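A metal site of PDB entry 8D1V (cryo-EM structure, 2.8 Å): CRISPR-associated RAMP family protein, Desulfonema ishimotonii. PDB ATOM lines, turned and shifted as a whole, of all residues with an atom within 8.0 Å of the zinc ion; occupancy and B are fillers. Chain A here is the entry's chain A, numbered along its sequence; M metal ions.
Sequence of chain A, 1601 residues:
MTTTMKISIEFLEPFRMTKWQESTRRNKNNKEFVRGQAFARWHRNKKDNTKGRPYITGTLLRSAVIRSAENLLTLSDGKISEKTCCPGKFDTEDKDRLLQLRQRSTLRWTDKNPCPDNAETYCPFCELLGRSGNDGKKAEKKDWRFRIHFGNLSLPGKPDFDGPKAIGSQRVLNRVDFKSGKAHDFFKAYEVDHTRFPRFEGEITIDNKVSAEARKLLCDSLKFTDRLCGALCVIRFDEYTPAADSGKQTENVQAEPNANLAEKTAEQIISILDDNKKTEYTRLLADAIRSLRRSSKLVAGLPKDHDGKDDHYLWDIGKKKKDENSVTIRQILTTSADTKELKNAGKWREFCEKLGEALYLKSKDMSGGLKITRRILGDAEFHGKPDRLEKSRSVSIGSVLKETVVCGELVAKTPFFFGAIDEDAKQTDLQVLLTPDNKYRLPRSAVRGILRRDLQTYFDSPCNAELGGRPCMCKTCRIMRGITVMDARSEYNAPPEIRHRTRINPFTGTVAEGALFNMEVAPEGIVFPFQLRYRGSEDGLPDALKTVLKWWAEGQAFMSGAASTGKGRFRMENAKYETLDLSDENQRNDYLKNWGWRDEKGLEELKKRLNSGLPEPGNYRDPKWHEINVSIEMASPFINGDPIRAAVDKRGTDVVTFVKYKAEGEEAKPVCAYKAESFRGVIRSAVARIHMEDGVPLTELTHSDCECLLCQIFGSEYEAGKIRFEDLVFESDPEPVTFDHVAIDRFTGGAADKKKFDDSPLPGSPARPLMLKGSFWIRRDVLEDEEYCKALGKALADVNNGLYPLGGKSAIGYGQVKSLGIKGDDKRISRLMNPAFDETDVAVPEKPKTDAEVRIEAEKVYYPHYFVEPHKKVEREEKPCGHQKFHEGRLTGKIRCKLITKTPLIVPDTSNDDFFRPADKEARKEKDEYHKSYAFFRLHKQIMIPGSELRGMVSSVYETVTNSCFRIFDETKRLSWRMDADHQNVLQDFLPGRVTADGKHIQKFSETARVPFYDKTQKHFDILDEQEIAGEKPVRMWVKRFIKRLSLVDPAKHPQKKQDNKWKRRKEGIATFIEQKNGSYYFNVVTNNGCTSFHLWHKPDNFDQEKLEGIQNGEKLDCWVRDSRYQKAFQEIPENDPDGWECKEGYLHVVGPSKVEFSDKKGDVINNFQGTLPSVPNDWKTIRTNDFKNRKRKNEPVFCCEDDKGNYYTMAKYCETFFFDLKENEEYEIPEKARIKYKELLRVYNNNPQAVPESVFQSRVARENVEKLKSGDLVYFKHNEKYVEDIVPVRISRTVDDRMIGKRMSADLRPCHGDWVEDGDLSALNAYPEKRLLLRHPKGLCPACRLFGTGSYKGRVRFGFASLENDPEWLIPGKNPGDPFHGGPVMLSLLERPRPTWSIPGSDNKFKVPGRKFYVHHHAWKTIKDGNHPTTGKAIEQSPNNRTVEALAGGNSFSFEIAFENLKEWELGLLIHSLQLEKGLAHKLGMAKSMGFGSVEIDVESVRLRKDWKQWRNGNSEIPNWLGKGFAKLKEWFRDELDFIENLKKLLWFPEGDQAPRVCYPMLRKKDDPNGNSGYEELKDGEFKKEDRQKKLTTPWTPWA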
ATOM      1  N   THR A  84      23.430  -4.022  30.327  1.00  0.00           N
ATOM      2  CA  THR A  84      22.624  -3.210  29.422  1.00  0.00           C
ATOM      3  C   THR A  84      21.213  -3.757  29.323  1.00  0.00           C
ATOM      4  O   THR A  84      20.926  -4.905  29.669  1.00  0.00           O
ATOM      5  CB  THR A  84      23.267  -3.157  28.040  1.00  0.00           C
ATOM      6  OG1 THR A  84      23.591  -4.480  27.603  1.00  0.00           O
ATOM      7  CG2 THR A  84      24.534  -2.318  28.073  1.00  0.00           C
ATOM      8  N   CYS A  85      20.301  -2.914  28.841  1.00  0.00           N
ATOM      9  CA  CYS A  85      18.918  -3.280  28.625  1.00  0.00           C
ATOM     10  C   CYS A  85      18.513  -2.929  27.204  1.00  0.00           C
ATOM     11  O   CYS A  85      18.895  -1.884  26.676  1.00  0.00           O
ATOM     12  CB  CYS A  85      17.978  -2.567  29.614  1.00  0.00           C
ATOM     13  SG  CYS A  85      18.207  -3.017  31.343  1.00  0.00           S
ATOM     14  N   CYS A  86      17.745  -3.819  26.577  1.00  0.00           N
ATOM     15  CA  CYS A  86      17.211  -3.537  25.260  1.00  0.00           C
ATOM     16  C   CYS A  86      16.038  -2.578  25.382  1.00  0.00           C
ATOM     17  O   CYS A  86      15.526  -2.339  26.473  1.00  0.00           O
ATOM     18  CB  CYS A  86      16.781  -4.820  24.568  1.00  0.00           C
ATOM     19  SG  CYS A  86      15.261  -5.545  25.193  1.00  0.00           S
ATOM     20  N   PRO A  87      15.599  -1.976  24.265  1.00  0.00           N
ATOM     21  CA  PRO A  87      14.486  -1.026  24.321  1.00  0.00           C
ATOM     22  C   PRO A  87      13.141  -1.640  24.665  1.00  0.00           C
ATOM     23  O   PRO A  87      12.170  -0.886  24.819  1.00  0.00           O
ATOM     24  CB  PRO A  87      14.474  -0.435  22.907  1.00  0.00           C
ATOM     25  CG  PRO A  87      15.090  -1.490  22.056  1.00  0.00           C
ATOM     26  CD  PRO A  87      16.155  -2.102  22.909  1.00  0.00           C
ATOM     27  N   GLY A  88      13.034  -2.950  24.799  1.00  0.00           N
ATOM     28  CA  GLY A  88      11.759  -3.595  25.025  1.00  0.00           C
ATOM     29  C   GLY A  88      11.016  -3.878  23.734  1.00  0.00           C
ATOM     30  O   GLY A  88      11.378  -3.402  22.663  1.00  0.00           O
ATOM     31  N   LYS A  89       9.960  -4.679  23.850  1.00  0.00           N
ATOM     32  CA  LYS A  89       9.214  -5.091  22.656  1.00  0.00           C
ATOM     33  C   LYS A  89       8.068  -4.130  22.344  1.00  0.00           C
ATOM     34  O   LYS A  89       8.064  -3.486  21.281  1.00  0.00           O
ATOM     35  CB  LYS A  89       8.684  -6.519  22.835  1.00  0.00           C
ATOM     36  CG  LYS A  89       8.171  -7.154  21.557  1.00  0.00           C
ATOM     37  CD  LYS A  89       7.702  -8.570  21.798  1.00  0.00           C
ATOM     38  CE  LYS A  89       7.042  -9.155  20.556  1.00  0.00           C
ATOM     39  NZ  LYS A  89       6.285 -10.398  20.879  1.00  0.00           N
ATOM     40  N   TRP A 109      17.175   4.451  24.139  1.00  0.00           N
ATOM     41  CA  TRP A 109      18.491   4.590  24.733  1.00  0.00           C
ATOM     42  C   TRP A 109      19.541   3.709  24.081  1.00  0.00           C
ATOM     43  O   TRP A 109      20.737   3.897  24.361  1.00  0.00           O
ATOM     44  CB  TRP A 109      18.427   4.294  26.238  1.00  0.00           C
ATOM     45  CG  TRP A 109      17.891   2.938  26.578  1.00  0.00           C
ATOM     46  CD1 TRP A 109      18.592   1.768  26.622  1.00  0.00           C
ATOM     47  CD2 TRP A 109      16.551   2.615  26.930  1.00  0.00           C
ATOM     48  NE1 TRP A 109      17.763   0.739  26.968  1.00  0.00           N
ATOM     49  CE2 TRP A 109      16.506   1.224  27.163  1.00  0.00           C
ATOM     50  CE3 TRP A 109      15.369   3.360  27.067  1.00  0.00           C
ATOM     51  CZ2 TRP A 109      15.328   0.573  27.533  1.00  0.00           C
ATOM     52  CZ3 TRP A 109      14.211   2.711  27.429  1.00  0.00           C
ATOM     53  CH2 TRP A 109      14.197   1.330  27.657  1.00  0.00           C
ATOM     54  N   LYS A 112      20.226  -1.625  20.049  1.00  0.00           N
ATOM     55  CA  LYS A 112      20.149  -3.078  20.078  1.00  0.00           C
ATOM     56  C   LYS A 112      18.707  -3.540  19.894  1.00  0.00           C
ATOM     57  O   LYS A 112      17.763  -2.878  20.325  1.00  0.00           O
ATOM     58  CB  LYS A 112      20.691  -3.607  21.408  1.00  0.00           C
ATOM     59  CG  LYS A 112      20.677  -5.124  21.522  1.00  0.00           C
ATOM     60  CD  LYS A 112      21.349  -5.549  22.816  1.00  0.00           C
ATOM     61  CE  LYS A 112      20.479  -5.245  24.024  1.00  0.00           C
ATOM     62  NZ  LYS A 112      21.083  -5.766  25.273  1.00  0.00           N
ATOM     63  N   ASN A 113      18.549  -4.687  19.243  1.00  0.00           N
ATOM     64  CA  ASN A 113      17.218  -5.253  19.074  1.00  0.00           C
ATOM     65  C   ASN A 113      16.707  -5.751  20.423  1.00  0.00           C
ATOM     66  O   ASN A 113      17.496  -6.072  21.311  1.00  0.00           O
ATOM     67  CB  ASN A 113      17.248  -6.386  18.059  1.00  0.00           C
ATOM     68  CG  ASN A 113      18.121  -6.074  16.846  1.00  0.00           C
ATOM     69  OD1 ASN A 113      19.101  -6.763  16.568  1.00  0.00           O
ATOM     70  ND2 ASN A 113      17.776  -5.001  16.136  1.00  0.00           N
ATOM     71  N   PRO A 114      15.394  -5.810  20.618  1.00  0.00           N
ATOM     72  CA  PRO A 114      14.831  -6.349  21.870  1.00  0.00           C
ATOM     73  C   PRO A 114      15.213  -7.806  22.076  1.00  0.00           C
ATOM     74  O   PRO A 114      15.632  -8.492  21.145  1.00  0.00           O
ATOM     75  CB  PRO A 114      13.255  -6.173  21.628  1.00  0.00           C
ATOM     76  CG  PRO A 114      13.546  -5.244  21.131  1.00  0.00           C
ATOM     77  CD  PRO A 114      14.175  -6.097  20.020  1.00  0.00           C
ATOM     78  N   CYS A 115      15.089  -8.267  23.320  1.00  0.00           N
ATOM     79  CA  CYS A 115      15.384  -9.658  23.616  1.00  0.00           C
ATOM     80  C   CYS A 115      14.446 -10.568  22.839  1.00  0.00           C
ATOM     81  O   CYS A 115      13.235 -10.303  22.777  1.00  0.00           O
ATOM     82  CB  CYS A 115      15.233  -9.915  25.123  1.00  0.00           C
ATOM     83  SG  CYS A 115      16.425  -9.034  26.142  1.00  0.00           S
ATOM     84  N   PRO A 116      14.956 -11.646  22.235  1.00  0.00           N
ATOM     85  CA  PRO A 116      14.076 -12.563  21.491  1.00  0.00           C
ATOM     86  C   PRO A 116      13.067 -13.232  22.420  1.00  0.00           C
ATOM     87  O   PRO A 116      13.352 -13.513  23.581  1.00  0.00           O
ATOM     88  CB  PRO A 116      15.042 -13.586  20.903  1.00  0.00           C
ATOM     89  CG  PRO A 116      16.236 -13.530  21.782  1.00  0.00           C
ATOM     90  CD  PRO A 116      16.352 -12.102  22.224  1.00  0.00           C
ATOM     91  N   THR A 121      17.328 -16.182  28.858  1.00  0.00           N
ATOM     92  CA  THR A 121      17.631 -15.058  29.736  1.00  0.00           C
ATOM     93  C   THR A 121      17.009 -13.787  29.173  1.00  0.00           C
ATOM     94  O   THR A 121      16.814 -13.637  27.971  1.00  0.00           O
ATOM     95  CB  THR A 121      19.149 -14.878  29.900  1.00  0.00           C
ATOM     96  OG1 THR A 121      19.397 -13.797  30.811  1.00  0.00           O
ATOM     97  CG2 THR A 121      19.793 -14.571  28.563  1.00  0.00           C
ATOM     98  N   TYR A 122      16.712 -12.847  30.079  1.00  0.00           N
ATOM     99  CA  TYR A 122      16.107 -11.576  29.713  1.00  0.00           C
ATOM    100  C   TYR A 122      16.855 -10.453  30.387  1.00  0.00           C
ATOM    101  O   TYR A 122      17.352 -10.615  31.513  1.00  0.00           O
ATOM    102  CB  TYR A 122      14.628 -11.529  30.120  1.00  0.00           C
ATOM    103  CG  TYR A 122      13.759 -12.553  29.417  1.00  0.00           C
ATOM    104  CD1 TYR A 122      13.520 -13.788  30.002  1.00  0.00           C
ATOM    105  CD2 TYR A 122      13.173 -12.276  28.194  1.00  0.00           C
ATOM    106  CE1 TYR A 122      12.727 -14.730  29.372  1.00  0.00           C
ATOM    107  CE2 TYR A 122      12.381 -13.214  27.555  1.00  0.00           C
ATOM    108  CZ  TYR A 122      12.162 -14.436  28.157  1.00  0.00           C
ATOM    109  OH  TYR A 122      11.370 -15.369  27.531  1.00  0.00           O
ATOM    110  N   CYS A 123      16.937  -9.303  29.724  1.00  0.00           N
ATOM    111  CA  CYS A 123      17.571  -8.125  30.295  1.00  0.00           C
ATOM    112  C   CYS A 123      16.694  -7.582  31.409  1.00  0.00           C
ATOM    113  O   CYS A 123      15.516  -7.946  31.501  1.00  0.00           O
ATOM    114  CB  CYS A 123      17.824  -7.064  29.231  1.00  0.00           C
ATOM    115  SG  CYS A 123      16.359  -6.123  28.750  1.00  0.00           S
ATOM    116  N   PRO A 124      17.243  -6.736  32.301  1.00  0.00           N
ATOM    117  CA  PRO A 124      16.470  -6.264  33.456  1.00  0.00           C
ATOM    118  C   PRO A 124      15.163  -5.556  33.079  1.00  0.00           C
ATOM    119  O   PRO A 124      14.164  -5.693  33.793  1.00  0.00           O
ATOM    120  CB  PRO A 124      17.435  -5.294  34.141  1.00  0.00           C
ATOM    121  CG  PRO A 124      18.786  -5.770  33.737  1.00  0.00           C
ATOM    122  CD  PRO A 124      18.636  -6.295  32.342  1.00  0.00           C
ATOM    123  N   PHE A 125      15.168  -4.817  31.970  1.00  0.00           N
ATOM    124  CA  PHE A 125      13.959  -4.153  31.525  1.00  0.00           C
ATOM    125  C   PHE A 125      12.864  -5.154  31.158  1.00  0.00           C
ATOM    126  O   PHE A 125      11.700  -4.962  31.503  1.00  0.00           O
ATOM    127  CB  PHE A 125      14.262  -3.237  30.335  1.00  0.00           C
ATOM    128  CG  PHE A 125      13.146  -2.284  30.010  1.00  0.00           C
ATOM    129  CD1 PHE A 125      12.696  -1.369  30.951  1.00  0.00           C
ATOM    130  CD2 PHE A 125      12.544  -2.316  28.772  1.00  0.00           C
ATOM    131  CE1 PHE A 125      11.673  -0.499  30.650  1.00  0.00           C
ATOM    132  CE2 PHE A 125      11.511  -1.444  28.470  1.00  0.00           C
ATOM    133  CZ  PHE A 125      11.080  -0.541  29.407  1.00  0.00           C
ATOM    134  N   CYS A 126      13.237  -6.220  30.453  1.00  0.00           N
ATOM    135  CA  CYS A 126      12.241  -7.234  30.097  1.00  0.00           C
ATOM    136  C   CYS A 126      11.714  -7.953  31.327  1.00  0.00           C
ATOM    137  O   CYS A 126      10.552  -8.379  31.359  1.00  0.00           O
ATOM    138  CB  CYS A 126      12.836  -8.232  29.095  1.00  0.00           C
ATOM    139  SG  CYS A 126      13.146  -7.550  27.466  1.00  0.00           S
ATOM    140  N   GLU A 127      12.555  -8.106  32.345  1.00  0.00           N
ATOM    141  CA  GLU A 127      12.071  -8.665  33.603  1.00  0.00           C
ATOM    142  C   GLU A 127      11.035  -7.750  34.249  1.00  0.00           C
ATOM    143  O   GLU A 127      10.020  -8.219  34.774  1.00  0.00           O
ATOM    144  CB  GLU A 127      13.257  -8.914  34.556  1.00  0.00           C
ATOM    145  CG  GLU A 127      14.013 -10.206  34.244  1.00  0.00           C
ATOM    146  CD  GLU A 127      15.360 -10.276  34.934  1.00  0.00           C
ATOM    147  OE1 GLU A 127      16.326  -9.663  34.436  1.00  0.00           O
ATOM    148  OE2 GLU A 127      15.452 -10.951  35.978  1.00  0.00           O
ATOM    149  N   LEU A 129       9.150  -5.650  32.578  1.00  0.00           N
ATOM    150  CA  LEU A 129       7.987  -5.709  31.700  1.00  0.00           C
ATOM    151  C   LEU A 129       7.151  -6.965  31.892  1.00  0.00           C
ATOM    152  O   LEU A 129       6.013  -6.997  31.421  1.00  0.00           O
ATOM    153  CB  LEU A 129       8.434  -5.619  30.246  1.00  0.00           C
ATOM    154  CG  LEU A 129       8.736  -4.215  29.739  1.00  0.00           C
ATOM    155  CD1 LEU A 129       9.151  -4.253  28.282  1.00  0.00           C
ATOM    156  CD2 LEU A 129       7.536  -3.318  29.931  1.00  0.00           C
ATOM    157  N   ARG A 131       7.952 -10.029  30.646  1.00  0.00           N
ATOM    158  CA  ARG A 131       8.065 -10.932  29.517  1.00  0.00           C
ATOM    159  C   ARG A 131       8.395 -12.349  29.989  1.00  0.00           C
ATOM    160  O   ARG A 131       9.234 -12.544  30.880  1.00  0.00           O
ATOM    161  CB  ARG A 131       9.130 -10.437  28.548  1.00  0.00           C
ATOM    162  CG  ARG A 131       8.930  -9.027  28.069  1.00  0.00           C
ATOM    163  CD  ARG A 131       9.965  -8.663  27.030  1.00  0.00           C
ATOM    164  NE  ARG A 131       9.829  -9.454  25.815  1.00  0.00           N
ATOM    165  CZ  ARG A 131      10.691  -9.454  24.815  1.00  0.00           C
ATOM    166  NH1 ARG A 131      11.781  -8.695  24.836  1.00  0.00           N
ATOM    167  NH2 ARG A 131      10.452 -10.229  23.755  1.00  0.00           N
HETATM  168 ZN    ZN M   1      15.353  -7.116  26.906  1.00  0.00          ZN
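The zinc ion is bound by the side-chain sulfur (SG) of Cys 126 (2.3 Å), the side-chain sulfur (SG) of Cys 123 (2.3 Å), the side-chain sulfur (SG) of Cys 115 (2.3 Å) and the side-chain sulfur (SG) of Cys 86 (2.3 Å). The zinc ion has four donor atoms within binding distance.
O of Cys 126 is in hydrogen-bond range of N of Arg 131 (3.2 Å). SG of Cys 123 sits close to N of Phe 125, at 3.7 Å. The guanidinium group of Arg 131 lies within hydrogen-bond range of the backbone carbonyl oxygen of Cys 115, 3.0 Å away. N of Gly 88 lies close to SG of Cys 86 (3.4 Å).
Along chain A the residues within 4 Å of the zinc ion span positions 86 to 126.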
